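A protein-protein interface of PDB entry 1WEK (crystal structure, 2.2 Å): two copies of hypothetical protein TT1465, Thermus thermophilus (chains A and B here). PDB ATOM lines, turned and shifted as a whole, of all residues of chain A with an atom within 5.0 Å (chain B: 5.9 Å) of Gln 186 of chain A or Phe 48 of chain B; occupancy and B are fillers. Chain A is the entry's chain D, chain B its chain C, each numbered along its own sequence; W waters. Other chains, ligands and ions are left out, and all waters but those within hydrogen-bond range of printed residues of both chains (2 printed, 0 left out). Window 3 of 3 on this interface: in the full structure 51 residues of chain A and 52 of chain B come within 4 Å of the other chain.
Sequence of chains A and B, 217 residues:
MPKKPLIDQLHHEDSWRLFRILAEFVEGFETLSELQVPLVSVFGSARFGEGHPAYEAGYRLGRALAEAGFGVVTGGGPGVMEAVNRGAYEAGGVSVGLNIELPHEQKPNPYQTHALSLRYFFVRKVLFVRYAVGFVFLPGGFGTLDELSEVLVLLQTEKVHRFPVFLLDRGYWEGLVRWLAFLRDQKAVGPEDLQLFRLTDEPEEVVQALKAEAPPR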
ATOM      1  N   PHE A 182     -18.536 -20.037  25.252  1.00  0.00           N
ATOM      2  CA  PHE A 182     -17.918 -21.248  24.733  1.00  0.00           C
ATOM      3  C   PHE A 182     -17.972 -21.187  23.200  1.00  0.00           C
ATOM      4  O   PHE A 182     -16.986 -21.480  22.515  1.00  0.00           O
ATOM      5  CB  PHE A 182     -18.676 -22.475  25.246  1.00  0.00           C
ATOM      6  CG  PHE A 182     -18.379 -23.737  24.490  1.00  0.00           C
ATOM      7  CD1 PHE A 182     -17.152 -24.377  24.621  1.00  0.00           C
ATOM      8  CD2 PHE A 182     -19.333 -24.290  23.643  1.00  0.00           C
ATOM      9  CE1 PHE A 182     -16.882 -25.556  23.917  1.00  0.00           C
ATOM     10  CE2 PHE A 182     -19.077 -25.463  22.935  1.00  0.00           C
ATOM     11  CZ  PHE A 182     -17.851 -26.098  23.070  1.00  0.00           C
ATOM     12  N   LEU A 183     -19.124 -20.788  22.670  1.00  0.00           N
ATOM     13  CA  LEU A 183     -19.297 -20.686  21.229  1.00  0.00           C
ATOM     14  C   LEU A 183     -18.268 -19.751  20.614  1.00  0.00           C
ATOM     15  O   LEU A 183     -17.695 -20.054  19.563  1.00  0.00           O
ATOM     16  CB  LEU A 183     -20.697 -20.183  20.894  1.00  0.00           C
ATOM     17  CG  LEU A 183     -21.839 -21.065  21.405  1.00  0.00           C
ATOM     18  CD1 LEU A 183     -23.177 -20.493  20.934  1.00  0.00           C
ATOM     19  CD2 LEU A 183     -21.641 -22.491  20.892  1.00  0.00           C
ATOM     20  N   ARG A 184     -18.031 -18.610  21.257  1.00  0.00           N
ATOM     21  CA  ARG A 184     -17.055 -17.671  20.723  1.00  0.00           C
ATOM     22  C   ARG A 184     -15.685 -18.302  20.804  1.00  0.00           C
ATOM     23  O   ARG A 184     -14.850 -18.076  19.942  1.00  0.00           O
ATOM     24  CB  ARG A 184     -17.050 -16.352  21.488  1.00  0.00           C
ATOM     25  CG  ARG A 184     -16.063 -15.345  20.909  1.00  0.00           C
ATOM     26  CD  ARG A 184     -16.017 -14.097  21.759  1.00  0.00           C
ATOM     27  NE  ARG A 184     -15.719 -14.433  23.149  1.00  0.00           N
ATOM     28  CZ  ARG A 184     -15.967 -13.636  24.188  1.00  0.00           C
ATOM     29  NH1 ARG A 184     -16.522 -12.443  24.000  1.00  0.00           N
ATOM     30  NH2 ARG A 184     -15.666 -14.040  25.419  1.00  0.00           N
ATOM     31  N   ASP A 185     -15.445 -19.083  21.854  1.00  0.00           N
ATOM     32  CA  ASP A 185     -14.159 -19.744  21.984  1.00  0.00           C
ATOM     33  C   ASP A 185     -14.058 -20.720  20.824  1.00  0.00           C
ATOM     34  O   ASP A 185     -12.999 -20.879  20.219  1.00  0.00           O
ATOM     35  CB  ASP A 185     -14.046 -20.505  23.310  1.00  0.00           C
ATOM     36  CG  ASP A 185     -13.889 -19.576  24.513  1.00  0.00           C
ATOM     37  OD1 ASP A 185     -13.307 -18.481  24.346  1.00  0.00           O
ATOM     38  OD2 ASP A 185     -14.333 -19.945  25.626  1.00  0.00           O
ATOM     39  N   GLN A 186     -15.181 -21.353  20.503  1.00  0.00           N
ATOM     40  CA  GLN A 186     -15.232 -22.319  19.414  1.00  0.00           C
ATOM     41  C   GLN A 186     -15.248 -21.677  18.028  1.00  0.00           C
ATOM     42  O   GLN A 186     -15.209 -22.381  17.024  1.00  0.00           O
ATOM     43  CB  GLN A 186     -16.459 -23.207  19.565  1.00  0.00           C
ATOM     44  CG  GLN A 186     -16.447 -24.050  20.800  1.00  0.00           C
ATOM     45  CD  GLN A 186     -15.329 -25.058  20.783  1.00  0.00           C
ATOM     46  OE1 GLN A 186     -15.235 -25.882  19.880  1.00  0.00           O
ATOM     47  NE2 GLN A 186     -14.472 -25.001  21.787  1.00  0.00           N
ATOM     48  N   LYS A 187     -15.296 -20.349  17.977  1.00  0.00           N
ATOM     49  CA  LYS A 187     -15.328 -19.614  16.706  1.00  0.00           C
ATOM     50  C   LYS A 187     -16.666 -19.792  15.991  1.00  0.00           C
ATOM     51  O   LYS A 187     -16.791 -19.486  14.807  1.00  0.00           O
ATOM     52  CB  LYS A 187     -14.200 -20.076  15.771  1.00  0.00           C
ATOM     53  CG  LYS A 187     -12.840 -19.424  15.984  1.00  0.00           C
ATOM     54  CD  LYS A 187     -12.275 -19.710  17.365  1.00  0.00           C
ATOM     55  CE  LYS A 187     -10.818 -19.283  17.439  1.00  0.00           C
ATOM     56  NZ  LYS A 187     -10.628 -17.891  16.963  1.00  0.00           N
ATOM     57  N   ALA A 188     -17.661 -20.305  16.710  1.00  0.00           N
ATOM     58  CA  ALA A 188     -18.989 -20.514  16.140  1.00  0.00           C
ATOM     59  C   ALA A 188     -19.650 -19.152  16.003  1.00  0.00           C
ATOM     60  O   ALA A 188     -20.616 -18.983  15.260  1.00  0.00           O
ATOM     61  CB  ALA A 188     -19.817 -21.417  17.050  1.00  0.00           C
ATOM     62  N   SER B  45     -23.529 -25.137  12.164  1.00  0.00           N
ATOM     63  CA  SER B  45     -22.708 -23.960  11.892  1.00  0.00           C
ATOM     64  C   SER B  45     -22.454 -23.686  10.413  1.00  0.00           C
ATOM     65  O   SER B  45     -22.257 -24.613   9.609  1.00  0.00           O
ATOM     66  CB  SER B  45     -21.357 -24.094  12.586  1.00  0.00           C
ATOM     67  OG  SER B  45     -20.513 -23.015  12.229  1.00  0.00           O
ATOM     68  N   ALA B  46     -22.448 -22.404  10.063  1.00  0.00           N
ATOM     69  CA  ALA B  46     -22.181 -21.977   8.697  1.00  0.00           C
ATOM     70  C   ALA B  46     -20.706 -21.631   8.562  1.00  0.00           C
ATOM     71  O   ALA B  46     -20.253 -21.232   7.487  1.00  0.00           O
ATOM     72  CB  ALA B  46     -23.012 -20.762   8.361  1.00  0.00           C
ATOM     73  N   ARG B  47     -19.957 -21.795   9.648  1.00  0.00           N
ATOM     74  CA  ARG B  47     -18.535 -21.462   9.652  1.00  0.00           C
ATOM     75  C   ARG B  47     -17.573 -22.644   9.597  1.00  0.00           C
ATOM     76  O   ARG B  47     -16.484 -22.532   9.037  1.00  0.00           O
ATOM     77  CB  ARG B  47     -18.202 -20.617  10.890  1.00  0.00           C
ATOM     78  CG  ARG B  47     -18.817 -19.213  10.932  1.00  0.00           C
ATOM     79  CD  ARG B  47     -18.333 -18.490  12.187  1.00  0.00           C
ATOM     80  NE  ARG B  47     -18.632 -17.056  12.245  1.00  0.00           N
ATOM     81  CZ  ARG B  47     -19.810 -16.538  12.577  1.00  0.00           C
ATOM     82  NH1 ARG B  47     -20.825 -17.336  12.877  1.00  0.00           N
ATOM     83  NH2 ARG B  47     -19.967 -15.223  12.648  1.00  0.00           N
ATOM     84  N   PHE B  48     -17.965 -23.772  10.175  1.00  0.00           N
ATOM     85  CA  PHE B  48     -17.102 -24.945  10.203  1.00  0.00           C
ATOM     86  C   PHE B  48     -17.062 -25.645   8.852  1.00  0.00           C
ATOM     87  O   PHE B  48     -18.031 -26.300   8.447  1.00  0.00           O
ATOM     88  CB  PHE B  48     -17.578 -25.918  11.290  1.00  0.00           C
ATOM     89  CG  PHE B  48     -17.687 -25.297  12.667  1.00  0.00           C
ATOM     90  CD1 PHE B  48     -18.539 -25.846  13.624  1.00  0.00           C
ATOM     91  CD2 PHE B  48     -16.957 -24.158  13.002  1.00  0.00           C
ATOM     92  CE1 PHE B  48     -18.668 -25.271  14.894  1.00  0.00           C
ATOM     93  CE2 PHE B  48     -17.076 -23.576  14.262  1.00  0.00           C
ATOM     94  CZ  PHE B  48     -17.934 -24.132  15.212  1.00  0.00           C
ATOM     95  N   GLY B  49     -15.932 -25.501   8.159  1.00  0.00           N
ATOM     96  CA  GLY B  49     -15.759 -26.117   6.856  1.00  0.00           C
ATOM     97  C   GLY B  49     -15.056 -27.463   6.909  1.00  0.00           C
ATOM     98  O   GLY B  49     -14.931 -28.070   7.977  1.00  0.00           O
ATOM     99  N   GLU B  50     -14.594 -27.918   5.745  1.00  0.00           N
ATOM    100  CA  GLU B  50     -13.897 -29.199   5.588  1.00  0.00           C
ATOM    101  C   GLU B  50     -12.733 -29.396   6.551  1.00  0.00           C
ATOM    102  O   GLU B  50     -11.815 -28.579   6.590  1.00  0.00           O
ATOM    103  CB  GLU B  50     -13.354 -29.330   4.168  1.00  0.00           C
ATOM    104  CG  GLU B  50     -14.390 -29.258   3.068  1.00  0.00           C
ATOM    105  CD  GLU B  50     -13.772 -29.453   1.693  1.00  0.00           C
ATOM    106  OE1 GLU B  50     -14.525 -29.511   0.695  1.00  0.00           O
ATOM    107  OE2 GLU B  50     -12.529 -29.549   1.610  1.00  0.00           O
ATOM    108  N   HIS B  52     -13.070 -29.638   9.835  1.00  0.00           N
ATOM    109  CA  HIS B  52     -13.613 -29.355  11.151  1.00  0.00           C
ATOM    110  C   HIS B  52     -14.505 -30.550  11.499  1.00  0.00           C
ATOM    111  O   HIS B  52     -15.280 -31.019  10.667  1.00  0.00           O
ATOM    112  CB  HIS B  52     -14.429 -28.056  11.117  1.00  0.00           C
ATOM    113  CG  HIS B  52     -14.781 -27.525  12.473  1.00  0.00           C
ATOM    114  ND1 HIS B  52     -15.630 -28.187  13.335  1.00  0.00           N
ATOM    115  CD2 HIS B  52     -14.375 -26.411  13.126  1.00  0.00           C
ATOM    116  CE1 HIS B  52     -15.731 -27.503  14.461  1.00  0.00           C
ATOM    117  NE2 HIS B  52     -14.980 -26.421  14.359  1.00  0.00           N
ATOM    118  N   ALA B  54     -17.178 -30.831  12.996  1.00  0.00           N
ATOM    119  CA  ALA B  54     -18.570 -30.519  12.708  1.00  0.00           C
ATOM    120  C   ALA B  54     -18.892 -30.830  11.248  1.00  0.00           C
ATOM    121  O   ALA B  54     -19.884 -31.502  10.953  1.00  0.00           O
ATOM    122  CB  ALA B  54     -18.846 -29.045  13.016  1.00  0.00           C
ATOM    123  N   TYR B  55     -18.042 -30.354  10.343  1.00  0.00           N
ATOM    124  CA  TYR B  55     -18.234 -30.575   8.915  1.00  0.00           C
ATOM    125  C   TYR B  55     -18.206 -32.056   8.546  1.00  0.00           C
ATOM    126  O   TYR B  55     -19.019 -32.532   7.750  1.00  0.00           O
ATOM    127  CB  TYR B  55     -17.151 -29.849   8.122  1.00  0.00           C
ATOM    128  CG  TYR B  55     -17.402 -29.800   6.627  1.00  0.00           C
ATOM    129  CD1 TYR B  55     -18.045 -28.707   6.040  1.00  0.00           C
ATOM    130  CD2 TYR B  55     -16.981 -30.837   5.799  1.00  0.00           C
ATOM    131  CE1 TYR B  55     -18.251 -28.646   4.661  1.00  0.00           C
ATOM    132  CE2 TYR B  55     -17.186 -30.790   4.422  1.00  0.00           C
ATOM    133  CZ  TYR B  55     -17.817 -29.693   3.857  1.00  0.00           C
ATOM    134  OH  TYR B  55     -17.985 -29.639   2.490  1.00  0.00           O
ATOM    135  N   PRO B  78     -22.983 -22.443   3.497  1.00  0.00           N
ATOM    136  CA  PRO B  78     -21.694 -23.124   3.647  1.00  0.00           C
ATOM    137  C   PRO B  78     -21.580 -23.834   4.990  1.00  0.00           C
ATOM    138  O   PRO B  78     -22.574 -24.037   5.683  1.00  0.00           O
ATOM    139  CB  PRO B  78     -20.698 -21.984   3.522  1.00  0.00           C
ATOM    140  CG  PRO B  78     -21.409 -20.877   4.285  1.00  0.00           C
ATOM    141  CD  PRO B  78     -22.872 -21.010   3.845  1.00  0.00           C
ATOM    142  N   GLY B  79     -20.359 -24.216   5.345  1.00  0.00           N
ATOM    143  CA  GLY B  79     -20.132 -24.887   6.611  1.00  0.00           C
ATOM    144  C   GLY B  79     -20.817 -26.232   6.761  1.00  0.00           C
ATOM    145  O   GLY B  79     -20.873 -27.019   5.820  1.00  0.00           O
ATOM    146  N   VAL B  80     -21.332 -26.505   7.954  1.00  0.00           N
ATOM    147  CA  VAL B  80     -21.991 -27.784   8.208  1.00  0.00           C
ATOM    148  C   VAL B  80     -23.218 -27.992   7.306  1.00  0.00           C
ATOM    149  O   VAL B  80     -23.628 -29.121   7.039  1.00  0.00           O
ATOM    150  CB  VAL B  80     -22.403 -27.902   9.696  1.00  0.00           C
ATOM    151  CG1 VAL B  80     -23.147 -29.196   9.941  1.00  0.00           C
ATOM    152  CG2 VAL B  80     -21.178 -27.847  10.563  1.00  0.00           C
ATOM    153  N   ALA B  83     -21.925 -29.309   4.176  1.00  0.00           N
ATOM    154  CA  ALA B  83     -21.483 -30.649   4.509  1.00  0.00           C
ATOM    155  C   ALA B  83     -22.660 -31.626   4.468  1.00  0.00           C
ATOM    156  O   ALA B  83     -22.565 -32.709   3.881  1.00  0.00           O
ATOM    157  CB  ALA B  83     -20.835 -30.660   5.886  1.00  0.00           C
ATOM    158  N   PRO B 139     -23.283 -28.823  15.859  1.00  0.00           N
ATOM    159  CA  PRO B 139     -22.603 -27.679  16.484  1.00  0.00           C
ATOM    160  C   PRO B 139     -22.692 -26.425  15.613  1.00  0.00           C
ATOM    161  O   PRO B 139     -22.383 -26.452  14.419  1.00  0.00           O
ATOM    162  CB  PRO B 139     -21.162 -28.171  16.639  1.00  0.00           C
ATOM    163  CG  PRO B 139     -21.317 -29.644  16.802  1.00  0.00           C
ATOM    164  CD  PRO B 139     -22.367 -29.975  15.751  1.00  0.00           C
ATOM    165  N   GLY B 140     -23.130 -25.328  16.211  1.00  0.00           N
ATOM    166  CA  GLY B 140     -23.244 -24.091  15.462  1.00  0.00           C
ATOM    167  C   GLY B 140     -23.309 -22.921  16.407  1.00  0.00           C
ATOM    168  O   GLY B 140     -23.065 -23.083  17.607  1.00  0.00           O
ATOM    169  N   TYR B 172     -20.466 -30.768  22.814  1.00  0.00           N
ATOM    170  CA  TYR B 172     -20.736 -29.393  22.404  1.00  0.00           C
ATOM    171  C   TYR B 172     -22.038 -28.796  22.963  1.00  0.00           C
ATOM    172  O   TYR B 172     -22.081 -27.616  23.307  1.00  0.00           O
ATOM    173  CB  TYR B 172     -20.765 -29.323  20.874  1.00  0.00           C
ATOM    174  CG  TYR B 172     -20.698 -27.928  20.301  1.00  0.00           C
ATOM    175  CD1 TYR B 172     -19.492 -27.405  19.844  1.00  0.00           C
ATOM    176  CD2 TYR B 172     -21.850 -27.136  20.188  1.00  0.00           C
ATOM    177  CE1 TYR B 172     -19.421 -26.136  19.283  1.00  0.00           C
ATOM    178  CE2 TYR B 172     -21.793 -25.864  19.632  1.00  0.00           C
ATOM    179  CZ  TYR B 172     -20.569 -25.369  19.177  1.00  0.00           C
ATOM    180  OH  TYR B 172     -20.486 -24.106  18.615  1.00  0.00           O
HETATM  181  O   HOH W   1     -23.314 -17.988  14.870  1.00  0.00           O
HETATM  182  O   HOH W   2     -21.326 -20.873  13.599  1.00  0.00           O
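Of the 16 printed residues of chain B, 4 touch a printed residue of chain A.
Hydrophobic or aromatic side chains of chain B within 4 Å of the printed part of chain A: Phe 48 and Tyr 172.
Of the 7 printed residues of chain A, 5 touch a printed residue of chain B.
Hydrophobic or aromatic side chains of chain A that line the printed part of chain B: Phe 182, Leu 183 and Ala 188.
The guanidinium group (NH1) of Arg 47 of chain B lies within hydrogen-bond range of the backbone carbonyl oxygen (O) of Ala 188 of chain A (2.9 Å).
Among the printed residues, merely in contact across the chains: Phe 182 of chain A with Tyr 172 of chain B (3.7 Å), Leu 183 of chain A with Gly 140 of chain B (3.6 Å), Leu 183 of chain A with Tyr 172 of chain B (3.0 Å), Gln 186 of chain A with Phe 48 of chain B (3.5 Å), Gln 186 of chain A with Tyr 172 of chain B (3.9 Å), Lys 187 of chain A with Arg 47 of chain B (3.2 Å), Ala 188 of chain A with Phe 48 of chain B (3.8 Å), Ala 188 of chain A with Gly 140 of chain B (3.7 Å) and Ala 188 of chain A with Tyr 172 of chain B (3.2 Å).
No position is printed for both chains.
Of the 10 pairs that touch across the chains among the printed residues, none has its exchanged pair printed and touching as well.
Of the printed residues of chain B, Leu 183 of chain A touches Gly 140 (3.6 Å) and Tyr 172 (3.0 Å).
Of chain B, only Phe 48 (3.5 Å) and Tyr 172 (3.9 Å) come within 4 Å of Gln 186 of chain A.
Of the printed residues of chain B, Ala 188 of chain A touches Arg 47 (2.9 Å), Phe 48 (3.8 Å), Gly 140 (3.7 Å) and Tyr 172 (3.2 Å).
Gly 79 of chain B touches none of the printed residues of chain A.
Of the printed residues of chain A, Gly 140 of chain B touches Leu 183 and Ala 188.
Of the printed residues of chain A, Tyr 172 of chain B touches Phe 182, Leu 183, Gln 186 and Ala 188.
The nearest residue of chain A that does not touch Phe 48 of chain B is Lys 187 of chain A (4.1 Å).
The side-chain hydroxyl (OG) of Ser 45 of chain B sits at hydrogen-bond distance from the backbone NH (N) of Arg 47 of chain B (2.9 Å).
The side-chain hydroxyl (OH) of Tyr 172 of chain B sits at hydrogen-bond distance from the backbone carbonyl oxygen (O) of Gly 140 of chain B (3.0 Å).
N of Phe 48 of chain B sits at hydrogen-bond distance from OG of Ser 45 of chain B, 3.4 Å away.
The backbone carbonyl oxygen (O) of Leu 183 of chain A lies within hydrogen-bond range of the backbone NH (N) of Ala 188 of chain A, 2.9 Å away.
O of Phe 48 of chain B sits at hydrogen-bond distance from N of Val 80 of chain B (3.3 Å).
Water W2 lies within hydrogen-bond range of O of Ala 188 of chain A (2.6 Å) and OG of Ser 45 of chain B (2.7 Å).
Water W1 bridges the backbone carbonyl oxygen of Ala 188 of chain A (2.9 Å) and the guanidinium group of Arg 47 of chain B (3.3 Å).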
